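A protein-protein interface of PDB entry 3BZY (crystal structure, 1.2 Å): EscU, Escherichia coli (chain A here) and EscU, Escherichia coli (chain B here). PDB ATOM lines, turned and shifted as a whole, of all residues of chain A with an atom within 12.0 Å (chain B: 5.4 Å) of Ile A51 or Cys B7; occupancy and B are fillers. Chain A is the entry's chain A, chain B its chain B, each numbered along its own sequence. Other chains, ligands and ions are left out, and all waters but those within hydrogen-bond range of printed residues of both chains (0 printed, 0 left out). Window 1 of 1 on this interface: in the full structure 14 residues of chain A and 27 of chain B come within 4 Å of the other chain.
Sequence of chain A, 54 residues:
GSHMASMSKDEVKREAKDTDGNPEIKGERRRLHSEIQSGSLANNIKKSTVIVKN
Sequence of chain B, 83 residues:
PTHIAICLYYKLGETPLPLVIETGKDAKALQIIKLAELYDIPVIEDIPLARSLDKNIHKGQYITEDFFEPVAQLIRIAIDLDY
The side-chain hydroxyl of Ser A48 sits close to the side-chain sulfur of Cys B7, at 3.3 Å.
The backbone NH (N) of Thr A49 is in hydrogen-bond range of the backbone carbonyl oxygen (O) of Leu B8 (2.8 Å).
The backbone carbonyl oxygen (O) of Val A50 sits at hydrogen-bond distance from the backbone NH (N) of Leu B8.
The backbone NH (N) of Ile A51 sits at hydrogen-bond distance from the backbone carbonyl oxygen (O) of Pro B42.
The backbone carbonyl oxygen (O) of Ile A51 is in hydrogen-bond range of the backbone NH (N) of Ile B44 (2.9 Å).
N of Ile B6 lies within hydrogen-bond range of O of Val A52 (2.9 Å).
The backbone NH of Lys A53 lies within hydrogen-bond range of the backbone carbonyl oxygen of Ile B44 (2.9 Å).
The side-chain carboxylate (OE1) of Glu B22 lies close to the side-chain amide nitrogen (ND2) of Asn A44 (2.2 Å).
The backbone carbonyl oxygen (O) of Ser A40 lies close to the side-chain amide nitrogen (ND2) of Asn A44 (3.4 Å).
O of Ile A45 is in hydrogen-bond range of OG of Ser A48 (2.8 Å).
The backbone NH (N) of Ile B21 is in hydrogen-bond range of the backbone carbonyl oxygen (O) of Cys B7, 2.9 Å away.
N of Cys B7 is in hydrogen-bond range of O of Glu B22 (2.9 Å).
The backbone NH (N) of Tyr B9 sits at hydrogen-bond distance from the backbone carbonyl oxygen (O) of Leu B19 (2.9 Å).
The backbone carbonyl oxygen (O) of Ala B36 lies within hydrogen-bond range of the backbone NH (N) of Ile B41 (2.9 Å).
Among the printed residues, merely in contact across the chains: Ser A40 with Glu B22 (3.9 Å), Leu A41 with Glu B22 (3.7 Å), Asn A44 with Ile B21 (3.2 Å), Ile A45 with Cys B7 (3.7 Å), Ile A45 with Ile B32 (3.9 Å), Ile A45 with Ala B36 (3.7 Å), Ile A45 with Ile B41 (3.4 Å), Lys A46 with Ile B41 (3.6 Å), Lys A47 with Tyr B9 (3.2 Å), Ser A48 with Leu B8 (3.7 Å), Ser A48 with Ile B41 (3.5 Å), Thr A49 with Tyr B9 (3.5 Å), Thr A49 with Pro B42 (3.6 Å), Val A50 with Ile B6 (3.9 Å), Val A50 with Cys B7 (3.8 Å), Val A50 with Pro B42 (3.5 Å), Val A50 with Ile B44 (3.95 Å), Ile A51 with Ile B6 (3.3 Å), Ile A51 with Cys B7 (3.95 Å), Ile A51 with Ala B36 (3.6 Å), Ile A51 with Ile B41 (3.9 Å), Ile A51 with Val B43 (3.4 Å), Val A52 with Ala B5 (3.5 Å), Val A52 with Leu B8 (3.9 Å), Val A52 with Ile B44 (3.3 Å) and Lys A53 with Val B43 (3.5 Å).
Ala A42 touches none of the printed residues of chain B.
Of the printed residues of chain B, Asn A44 touches Ile B21 and Glu B22.
Of the printed residues of chain B, Ile A45 touches Cys B7 (3.7 Å), Ile B32 (3.9 Å), Ala B36 (3.7 Å) and Ile B41 (3.4 Å).
Of the printed residues of chain B, Lys A46 touches Ile B41 (3.6 Å).
Printed residues of chain B within 4 Å of Lys A47: Tyr B9 (3.2 Å).
Of the printed residues of chain B, Ile A51 touches Ile B6 (3.3 Å), Cys B7 (3.95 Å), Ala B36 (3.6 Å), Ile B41 (3.9 Å), Pro B42 (2.9 Å), Val B43 (3.4 Å) and Ile B44 (2.9 Å).
Of the printed residues of chain B, Val A52 touches Ala B5 (3.5 Å), Ile B6 (2.9 Å), Leu B8 (3.9 Å) and Ile B44 (3.3 Å).
Printed residues of chain A within 4 Å of Cys B7: Ile A45 (3.7 Å), Ser A48 (3.1 Å), Val A50 (3.8 Å) and Ile A51 (3.95 Å).
No residue of chain A comes within 4 Å of Leu B19.
No residue of chain A comes within 4 Å of Val B20.
No residue of chain A comes within 4 Å of Thr B23.
Ile B33 touches none of the printed residues of chain A.
Of chain A, only Ile A45 (3.7 Å) and Ile A51 (3.6 Å) come within 4 Å of Ala B36.
Pro B42 touches just these residues of chain A: Thr A49 (3.6 Å), Val A50 (3.5 Å) and Ile A51 (2.9 Å).
The nearest printed residue of chain A that does not touch Cys B7 is Asn A44 (4.1 Å).
The nearest printed residue of chain A that does not touch Ile B41 is Thr A49 (4.1 Å).
Along chain A the printed residues that touch a printed residue of chain B span positions 40 to 53.
Of the 17 printed residues of chain B, 13 touch a printed residue of chain A.
Hydrophobic or aromatic side chains of chain B that line the printed part of chain A: Ile B6, Leu B8, Tyr B9, Ile B21, Ile B32, Ala B36, Ile B41, Pro B42, Val B43 and Ile B44.
Among the printed residues, 34 pairs touch across the chains.
Among the printed residues, no Asp or Glu carboxylate lies within 4 Å of a Lys or Arg side-chain nitrogen of the other chain.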
ATOM      1  N   GLY A  39     -10.612  17.585 -12.048  1.00  0.00           N
ATOM      2  CA  GLY A  39     -11.564  16.452 -11.948  1.00  0.00           C
ATOM      3  C   GLY A  39     -12.437  16.451 -10.705  1.00  0.00           C
ATOM      4  O   GLY A  39     -13.312  15.645 -10.656  1.00  0.00           O
ATOM      5  N   SER A  40     -12.159  17.284  -9.718  1.00  0.00           N
ATOM      6  CA  SER A  40     -12.892  17.346  -8.557  1.00  0.00           C
ATOM      7  C   SER A  40     -14.363  17.636  -8.882  1.00  0.00           C
ATOM      8  O   SER A  40     -15.145  17.055  -8.211  1.00  0.00           O
ATOM      9  CB  SER A  40     -12.266  18.286  -7.582  1.00  0.00           C
ATOM     10  OG  SER A  40     -12.303  19.714  -7.899  1.00  0.00           O
ATOM     11  N   LEU A  41     -14.632  18.582  -9.802  1.00  0.00           N
ATOM     12  CA  LEU A  41     -16.059  18.881 -10.130  1.00  0.00           C
ATOM     13  C   LEU A  41     -16.745  17.595 -10.528  1.00  0.00           C
ATOM     14  O   LEU A  41     -17.807  17.218 -10.024  1.00  0.00           O
ATOM     15  CB  LEU A  41     -16.143  19.937 -11.162  1.00  0.00           C
ATOM     16  CG  LEU A  41     -17.563  20.230 -11.681  1.00  0.00           C
ATOM     17  CD1 LEU A  41     -18.460  20.663 -10.499  1.00  0.00           C
ATOM     18  CD2 LEU A  41     -17.524  21.229 -12.807  1.00  0.00           C
ATOM     19  N   ALA A  42     -16.163  16.913 -11.532  1.00  0.00           N
ATOM     20  CA  ALA A  42     -16.795  15.723 -12.036  1.00  0.00           C
ATOM     21  C   ALA A  42     -16.917  14.620 -11.013  1.00  0.00           C
ATOM     22  O   ALA A  42     -17.933  13.908 -10.976  1.00  0.00           O
ATOM     23  CB  ALA A  42     -16.063  15.219 -13.325  1.00  0.00           C
ATOM     24  N   ASN A  43     -15.913  14.426 -10.207  1.00  0.00           N
ATOM     25  CA  ASN A  43     -16.000  13.409  -9.198  1.00  0.00           C
ATOM     26  C   ASN A  43     -17.103  13.744  -8.142  1.00  0.00           C
ATOM     27  O   ASN A  43     -17.805  12.798  -7.706  1.00  0.00           O
ATOM     28  CB  ASN A  43     -14.672  13.216  -8.467  1.00  0.00           C
ATOM     29  CG  ASN A  43     -13.637  12.496  -9.388  1.00  0.00           C
ATOM     30  OD1 ASN A  43     -14.039  11.756 -10.293  1.00  0.00           O
ATOM     31  ND2 ASN A  43     -12.426  12.712  -9.137  1.00  0.00           N
ATOM     32  N   ASN A  44     -17.223  15.015  -7.833  1.00  0.00           N
ATOM     33  CA  ASN A  44     -18.358  15.410  -6.884  1.00  0.00           C
ATOM     34  C   ASN A  44     -19.719  15.163  -7.519  1.00  0.00           C
ATOM     35  O   ASN A  44     -20.608  14.663  -6.823  1.00  0.00           O
ATOM     36  CB  ASN A  44     -18.151  16.860  -6.543  1.00  0.00           C
ATOM     37  CG  ASN A  44     -17.096  17.070  -5.491  1.00  0.00           C
ATOM     38  OD1 ASN A  44     -16.749  16.174  -4.766  1.00  0.00           O
ATOM     39  ND2 ASN A  44     -16.617  18.322  -5.431  1.00  0.00           N
ATOM     40  N   ILE A  45     -19.887  15.460  -8.814  1.00  0.00           N
ATOM     41  CA  ILE A  45     -21.178  15.211  -9.461  1.00  0.00           C
ATOM     42  C   ILE A  45     -21.406  13.724  -9.485  1.00  0.00           C
ATOM     43  O   ILE A  45     -22.523  13.272  -9.187  1.00  0.00           O
ATOM     44  CB  ILE A  45     -21.289  15.869 -10.789  1.00  0.00           C
ATOM     45  CG1 ILE A  45     -21.024  17.408 -10.748  1.00  0.00           C
ATOM     46  CG2 ILE A  45     -22.636  15.546 -11.454  1.00  0.00           C
ATOM     47  CD1 ILE A  45     -21.772  18.129  -9.714  1.00  0.00           C
ATOM     48  N   LYS A  46     -20.418  12.896  -9.850  1.00  0.00           N
ATOM     49  CA  LYS A  46     -20.698  11.497 -10.002  1.00  0.00           C
ATOM     50  C   LYS A  46     -21.164  10.846  -8.733  1.00  0.00           C
ATOM     51  O   LYS A  46     -21.988   9.936  -8.798  1.00  0.00           O
ATOM     52  CB  LYS A  46     -19.469  10.760 -10.592  1.00  0.00           C
ATOM     53  CG  LYS A  46     -19.773   9.270 -10.950  1.00  0.00           C
ATOM     54  CD  LYS A  46     -18.625   8.574 -11.558  1.00  0.00           C
ATOM     55  CE  LYS A  46     -17.435   8.514 -10.624  1.00  0.00           C
ATOM     56  N   LYS A  47     -20.686  11.310  -7.575  1.00  0.00           N
ATOM     57  CA  LYS A  47     -21.132  10.704  -6.287  1.00  0.00           C
ATOM     58  C   LYS A  47     -22.398  11.306  -5.654  1.00  0.00           C
ATOM     59  O   LYS A  47     -22.882  10.828  -4.653  1.00  0.00           O
ATOM     60  CB  LYS A  47     -20.027  10.709  -5.277  1.00  0.00           C
ATOM     61  CG  LYS A  47     -19.688  12.041  -4.710  1.00  0.00           C
ATOM     62  CD  LYS A  47     -18.622  11.815  -3.594  1.00  0.00           C
ATOM     63  CE  LYS A  47     -18.438  12.913  -2.729  1.00  0.00           C
ATOM     64  NZ  LYS A  47     -17.259  12.805  -1.819  1.00  0.00           N
ATOM     65  N   SER A  48     -22.896  12.351  -6.308  1.00  0.00           N
ATOM     66  CA  SER A  48     -23.954  13.031  -5.602  1.00  0.00           C
ATOM     67  C   SER A  48     -25.270  12.412  -5.737  1.00  0.00           C
ATOM     68  O   SER A  48     -25.534  11.441  -6.452  1.00  0.00           O
ATOM     69  CB  SER A  48     -23.985  14.394  -6.139  1.00  0.00           C
ATOM     70  OG  SER A  48     -24.436  14.372  -7.507  1.00  0.00           O
ATOM     71  N   THR A  49     -26.163  12.864  -4.840  1.00  0.00           N
ATOM     72  CA  THR A  49     -27.482  12.255  -4.654  1.00  0.00           C
ATOM     73  C   THR A  49     -28.542  12.898  -5.568  1.00  0.00           C
ATOM     74  O   THR A  49     -29.342  12.183  -6.182  1.00  0.00           O
ATOM     75  CB  THR A  49     -27.864  12.340  -3.154  1.00  0.00           C
ATOM     76  OG1 THR A  49     -26.791  11.876  -2.350  1.00  0.00           O
ATOM     77  CG2 THR A  49     -29.188  11.589  -2.899  1.00  0.00           C
ATOM     78  N   VAL A  50     -28.579  14.248  -5.606  1.00  0.00           N
ATOM     79  CA  VAL A  50     -29.607  14.886  -6.366  1.00  0.00           C
ATOM     80  C   VAL A  50     -29.103  16.292  -6.663  1.00  0.00           C
ATOM     81  O   VAL A  50     -28.356  16.871  -5.841  1.00  0.00           O
ATOM     82  CB  VAL A  50     -30.982  14.899  -5.596  1.00  0.00           C
ATOM     83  CG1 VAL A  50     -30.873  15.643  -4.220  1.00  0.00           C
ATOM     84  CG2 VAL A  50     -32.075  15.480  -6.494  1.00  0.00           C
ATOM     85  N   ILE A  51     -29.486  16.825  -7.807  1.00  0.00           N
ATOM     86  CA  ILE A  51     -29.169  18.209  -8.182  1.00  0.00           C
ATOM     87  C   ILE A  51     -30.481  18.966  -8.243  1.00  0.00           C
ATOM     88  O   ILE A  51     -31.440  18.502  -8.831  1.00  0.00           O
ATOM     89  CB  ILE A  51     -28.433  18.288  -9.449  1.00  0.00           C
ATOM     90  CG1 ILE A  51     -26.891  17.585  -9.088  1.00  0.00           C
ATOM     91  CG2 ILE A  51     -28.276  19.674 -10.007  1.00  0.00           C
ATOM     92  CD1 ILE A  51     -26.170  17.121 -10.214  1.00  0.00           C
ATOM     93  N   VAL A  52     -30.500  20.132  -7.651  1.00  0.00           N
ATOM     94  CA  VAL A  52     -31.629  21.088  -7.699  1.00  0.00           C
ATOM     95  C   VAL A  52     -31.255  22.203  -8.605  1.00  0.00           C
ATOM     96  O   VAL A  52     -30.197  22.801  -8.396  1.00  0.00           O
ATOM     97  CB  VAL A  52     -31.872  21.703  -6.335  1.00  0.00           C
ATOM     98  CG1 VAL A  52     -33.118  22.647  -6.411  1.00  0.00           C
ATOM     99  CG2 VAL A  52     -32.114  20.569  -5.330  1.00  0.00           C
ATOM    100  N   LYS A  53     -32.072  22.542  -9.565  1.00  0.00           N
ATOM    101  CA  LYS A  53     -31.832  23.616 -10.477  1.00  0.00           C
ATOM    102  C   LYS A  53     -33.003  24.564 -10.502  1.00  0.00           C
ATOM    103  O   LYS A  53     -34.126  24.265 -10.146  1.00  0.00           O
ATOM    104  CB  LYS A  53     -31.486  23.162 -11.915  1.00  0.00           C
ATOM    105  CG  LYS A  53     -32.626  22.467 -12.590  1.00  0.00           C
ATOM    106  CD  LYS A  53     -32.249  22.028 -14.039  1.00  0.00           C
ATOM    107  CE  LYS A  53     -32.100  23.140 -15.035  1.00  0.00           C
ATOM    108  NZ  LYS A  53     -33.445  23.758 -15.374  1.00  0.00           N
ATOM    109  N   ASN A  54     -32.709  25.790 -10.950  1.00  0.00           N
ATOM    110  CA  ASN A  54     -33.762  26.745 -11.346  1.00  0.00           C
ATOM    111  C   ASN A  54     -34.129  26.641 -12.842  1.00  0.00           C
ATOM    112  O   ASN A  54     -33.812  25.567 -13.383  1.00  0.00           O
ATOM    113  CB  ASN A  54     -33.395  28.176 -10.954  1.00  0.00           C
ATOM    114  CG  ASN A  54     -32.327  28.770 -11.795  1.00  0.00           C
ATOM    115  OD1 ASN A  54     -31.591  28.040 -12.446  1.00  0.00           O
ATOM    116  ND2 ASN A  54     -32.158  30.065 -11.757  1.00  0.00           N
ATOM    117  OXT ASN A  54     -34.650  27.636 -13.414  1.00  0.00           O
ATOM    118  N   ALA B   5     -27.337  25.666 -10.274  1.00  0.00           N
ATOM    119  CA  ALA B   5     -27.391  24.232  -9.973  1.00  0.00           C
ATOM    120  C   ALA B   5     -26.748  24.014  -8.618  1.00  0.00           C
ATOM    121  O   ALA B   5     -25.635  24.464  -8.365  1.00  0.00           O
ATOM    122  CB  ALA B   5     -26.700  23.394 -11.073  1.00  0.00           C
ATOM    123  N   ILE B   6     -27.447  23.262  -7.759  1.00  0.00           N
ATOM    124  CA  ILE B   6     -27.012  22.924  -6.408  1.00  0.00           C
ATOM    125  C   ILE B   6     -26.925  21.415  -6.329  1.00  0.00           C
ATOM    126  O   ILE B   6     -27.895  20.708  -6.531  1.00  0.00           O
ATOM    127  CB  ILE B   6     -27.976  23.440  -5.345  1.00  0.00           C
ATOM    128  CG1 ILE B   6     -28.269  24.956  -5.490  1.00  0.00           C
ATOM    129  CG2 ILE B   6     -27.449  23.117  -3.935  1.00  0.00           C
ATOM    130  CD1 ILE B   6     -27.149  25.838  -5.327  1.00  0.00           C
ATOM    131  N   CYS B   7     -25.727  20.899  -5.979  1.00  0.00           N
ATOM    132  CA  CYS B   7     -25.466  19.475  -5.924  1.00  0.00           C
ATOM    133  C   CYS B   7     -25.485  19.009  -4.446  1.00  0.00           C
ATOM    134  O   CYS B   7     -24.626  19.449  -3.682  1.00  0.00           O
ATOM    135  CB  CYS B   7     -24.048  19.208  -6.524  1.00  0.00           C
ATOM    136  SG  CYS B   7     -23.603  17.433  -6.532  1.00  0.00           S
ATOM    137  N   LEU B   8     -26.427  18.162  -4.123  1.00  0.00           N
ATOM    138  CA  LEU B   8     -26.595  17.658  -2.765  1.00  0.00           C
ATOM    139  C   LEU B   8     -26.093  16.233  -2.696  1.00  0.00           C
ATOM    140  O   LEU B   8     -26.369  15.382  -3.551  1.00  0.00           O
ATOM    141  CB  LEU B   8     -28.100  17.716  -2.395  1.00  0.00           C
ATOM    142  CG  LEU B   8     -28.597  19.120  -2.111  1.00  0.00           C
ATOM    143  CD1 LEU B   8     -30.126  19.156  -2.342  1.00  0.00           C
ATOM    144  CD2 LEU B   8     -28.281  19.569  -0.647  1.00  0.00           C
ATOM    145  N   TYR B   9     -25.451  15.920  -1.573  1.00  0.00           N
ATOM    146  CA  TYR B   9     -24.888  14.596  -1.274  1.00  0.00           C
ATOM    147  C   TYR B   9     -25.311  14.166   0.133  1.00  0.00           C
ATOM    148  O   TYR B   9     -25.136  14.907   1.102  1.00  0.00           O
ATOM    149  CB  TYR B   9     -23.368  14.642  -1.339  1.00  0.00           C
ATOM    150  CG  TYR B   9     -22.675  13.333  -1.002  1.00  0.00           C
ATOM    151  CD1 TYR B   9     -21.789  13.245   0.073  1.00  0.00           C
ATOM    152  CD2 TYR B   9     -22.884  12.180  -1.717  1.00  0.00           C
ATOM    153  CE1 TYR B   9     -21.069  12.069   0.358  1.00  0.00           C
ATOM    154  CE2 TYR B   9     -22.212  10.985  -1.403  1.00  0.00           C
ATOM    155  CZ  TYR B   9     -21.356  11.009  -0.381  1.00  0.00           C
ATOM    156  OH  TYR B   9     -20.707   9.732  -0.083  1.00  0.00           O
ATOM    157  N   LEU B  19     -25.313  17.462   2.458  1.00  0.00           N
ATOM    158  CA  LEU B  19     -24.236  18.378   2.219  1.00  0.00           C
ATOM    159  C   LEU B  19     -24.347  18.978   0.828  1.00  0.00           C
ATOM    160  O   LEU B  19     -24.567  18.233  -0.142  1.00  0.00           O
ATOM    161  CB  LEU B  19     -22.882  17.496   2.264  1.00  0.00           C
ATOM    162  CG  LEU B  19     -21.562  18.226   2.141  1.00  0.00           C
ATOM    163  CD1 LEU B  19     -21.282  19.292   3.207  1.00  0.00           C
ATOM    164  CD2 LEU B  19     -20.448  17.128   2.157  1.00  0.00           C
ATOM    165  N   VAL B  20     -24.133  20.272   0.698  1.00  0.00           N
ATOM    166  CA  VAL B  20     -23.997  20.911  -0.630  1.00  0.00           C
ATOM    167  C   VAL B  20     -22.532  20.724  -1.031  1.00  0.00           C
ATOM    168  O   VAL B  20     -21.648  21.377  -0.492  1.00  0.00           O
ATOM    169  CB  VAL B  20     -24.401  22.381  -0.603  1.00  0.00           C
ATOM    170  CG1 VAL B  20     -24.047  23.048  -1.924  1.00  0.00           C
ATOM    171  CG2 VAL B  20     -25.937  22.491  -0.366  1.00  0.00           C
ATOM    172  N   ILE B  21     -22.295  19.810  -1.936  1.00  0.00           N
ATOM    173  CA  ILE B  21     -20.866  19.521  -2.286  1.00  0.00           C
ATOM    174  C   ILE B  21     -20.403  20.280  -3.489  1.00  0.00           C
ATOM    175  O   ILE B  21     -19.169  20.420  -3.623  1.00  0.00           O
ATOM    176  CB  ILE B  21     -20.548  18.068  -2.443  1.00  0.00           C
ATOM    177  CG1 ILE B  21     -21.390  17.361  -3.556  1.00  0.00           C
ATOM    178  CG2 ILE B  21     -20.629  17.317  -1.094  1.00  0.00           C
ATOM    179  CD1 ILE B  21     -20.884  15.901  -3.852  1.00  0.00           C
ATOM    180  N   GLU B  22     -21.285  20.814  -4.298  1.00  0.00           N
ATOM    181  CA  GLU B  22     -20.925  21.699  -5.437  1.00  0.00           C
ATOM    182  C   GLU B  22     -22.060  22.549  -5.723  1.00  0.00           C
ATOM    183  O   GLU B  22     -23.238  22.217  -5.537  1.00  0.00           O
ATOM    184  CB  GLU B  22     -20.619  20.977  -6.766  1.00  0.00           C
ATOM    185  CG  GLU B  22     -19.449  20.055  -6.752  1.00  0.00           C
ATOM    186  CD  GLU B  22     -18.110  20.774  -6.791  1.00  0.00           C
ATOM    187  OE1 GLU B  22     -17.078  20.070  -6.747  1.00  0.00           O
ATOM    188  OE2 GLU B  22     -18.043  22.019  -6.984  1.00  0.00           O
ATOM    189  N   THR B  23     -21.752  23.717  -6.262  1.00  0.00           N
ATOM    190  CA  THR B  23     -22.706  24.697  -6.734  1.00  0.00           C
ATOM    191  C   THR B  23     -22.204  25.330  -7.983  1.00  0.00           C
ATOM    192  O   THR B  23     -20.963  25.382  -8.238  1.00  0.00           O
ATOM    193  CB  THR B  23     -22.987  25.783  -5.722  1.00  0.00           C
ATOM    194  OG1 THR B  23     -21.823  26.621  -5.605  1.00  0.00           O
ATOM    195  CG2 THR B  23     -23.384  25.340  -4.369  1.00  0.00           C
ATOM    196  N   ILE B  32     -22.535  21.545 -14.818  1.00  0.00           N
ATOM    197  CA  ILE B  32     -23.013  20.615 -13.802  1.00  0.00           C
ATOM    198  C   ILE B  32     -24.166  19.787 -14.331  1.00  0.00           C
ATOM    199  O   ILE B  32     -24.209  18.571 -14.092  1.00  0.00           O
ATOM    200  CB  ILE B  32     -23.419  21.334 -12.505  1.00  0.00           C
ATOM    201  CG1 ILE B  32     -22.175  21.862 -11.783  1.00  0.00           C
ATOM    202  CG2 ILE B  32     -24.284  20.517 -11.587  1.00  0.00           C
ATOM    203  CD1 ILE B  32     -22.437  22.817 -10.610  1.00  0.00           C
ATOM    204  N   ILE B  33     -25.104  20.416 -15.034  1.00  0.00           N
ATOM    205  CA  ILE B  33     -26.263  19.696 -15.604  1.00  0.00           C
ATOM    206  C   ILE B  33     -25.804  18.663 -16.622  1.00  0.00           C
ATOM    207  O   ILE B  33     -26.306  17.529 -16.685  1.00  0.00           O
ATOM    208  CB  ILE B  33     -27.283  20.685 -16.207  1.00  0.00           C
ATOM    209  CG1 ILE B  33     -27.919  21.485 -15.057  1.00  0.00           C
ATOM    210  CG2 ILE B  33     -28.292  19.955 -17.018  1.00  0.00           C
ATOM    211  CD1 ILE B  33     -28.381  20.720 -13.873  1.00  0.00           C
ATOM    212  N   ALA B  36     -24.380  15.827 -14.705  1.00  0.00           N
ATOM    213  CA  ALA B  36     -25.453  15.084 -14.110  1.00  0.00           C
ATOM    214  C   ALA B  36     -26.053  14.082 -15.091  1.00  0.00           C
ATOM    215  O   ALA B  36     -26.336  12.927 -14.757  1.00  0.00           O
ATOM    216  CB  ALA B  36     -26.526  16.030 -13.606  1.00  0.00           C
ATOM    217  N   ILE B  41     -27.389  11.371 -12.613  1.00  0.00           N
ATOM    218  CA  ILE B  41     -27.788  11.932 -11.328  1.00  0.00           C
ATOM    219  C   ILE B  41     -29.150  12.592 -11.525  1.00  0.00           C
ATOM    220  O   ILE B  41     -29.309  13.405 -12.422  1.00  0.00           O
ATOM    221  CB  ILE B  41     -26.792  12.975 -10.843  1.00  0.00           C
ATOM    222  CG1 ILE B  41     -25.341  12.454 -10.892  1.00  0.00           C
ATOM    223  CG2 ILE B  41     -27.171  13.476  -9.445  1.00  0.00           C
ATOM    224  CD1 ILE B  41     -25.124  11.229 -10.080  1.00  0.00           C
ATOM    225  N   PRO B  42     -30.121  12.294 -10.661  1.00  0.00           N
ATOM    226  CA  PRO B  42     -31.410  12.950 -10.778  1.00  0.00           C
ATOM    227  C   PRO B  42     -31.291  14.474 -10.636  1.00  0.00           C
ATOM    228  O   PRO B  42     -30.609  14.984  -9.742  1.00  0.00           O
ATOM    229  CB  PRO B  42     -32.230  12.381  -9.623  1.00  0.00           C
ATOM    230  CG  PRO B  42     -31.638  11.015  -9.408  1.00  0.00           C
ATOM    231  CD  PRO B  42     -30.119  11.260  -9.603  1.00  0.00           C
ATOM    232  N   VAL B  43     -31.962  15.188 -11.550  1.00  0.00           N
ATOM    233  CA  VAL B  43     -32.026  16.634 -11.569  1.00  0.00           C
ATOM    234  C   VAL B  43     -33.481  17.062 -11.429  1.00  0.00           C
ATOM    235  O   VAL B  43     -34.322  16.626 -12.187  1.00  0.00           O
ATOM    236  CB  VAL B  43     -31.454  17.208 -12.894  1.00  0.00           C
ATOM    237  CG1 VAL B  43     -31.606  18.720 -12.942  1.00  0.00           C
ATOM    238  CG2 VAL B  43     -29.965  16.798 -13.062  1.00  0.00           C
ATOM    239  N   ILE B  44     -33.729  17.897 -10.438  1.00  0.00           N
ATOM    240  CA  ILE B  44     -35.078  18.390 -10.095  1.00  0.00           C
ATOM    241  C   ILE B  44     -35.064  19.904 -10.268  1.00  0.00           C
ATOM    242  O   ILE B  44     -34.253  20.597  -9.683  1.00  0.00           O
ATOM    243  CB  ILE B  44     -35.529  17.926  -8.721  1.00  0.00           C
ATOM    244  CG1 ILE B  44     -35.526  16.371  -8.648  1.00  0.00           C
ATOM    245  CG2 ILE B  44     -36.861  18.564  -8.345  1.00  0.00           C
ATOM    246  CD1 ILE B  44     -35.915  15.686  -7.417  1.00  0.00           C
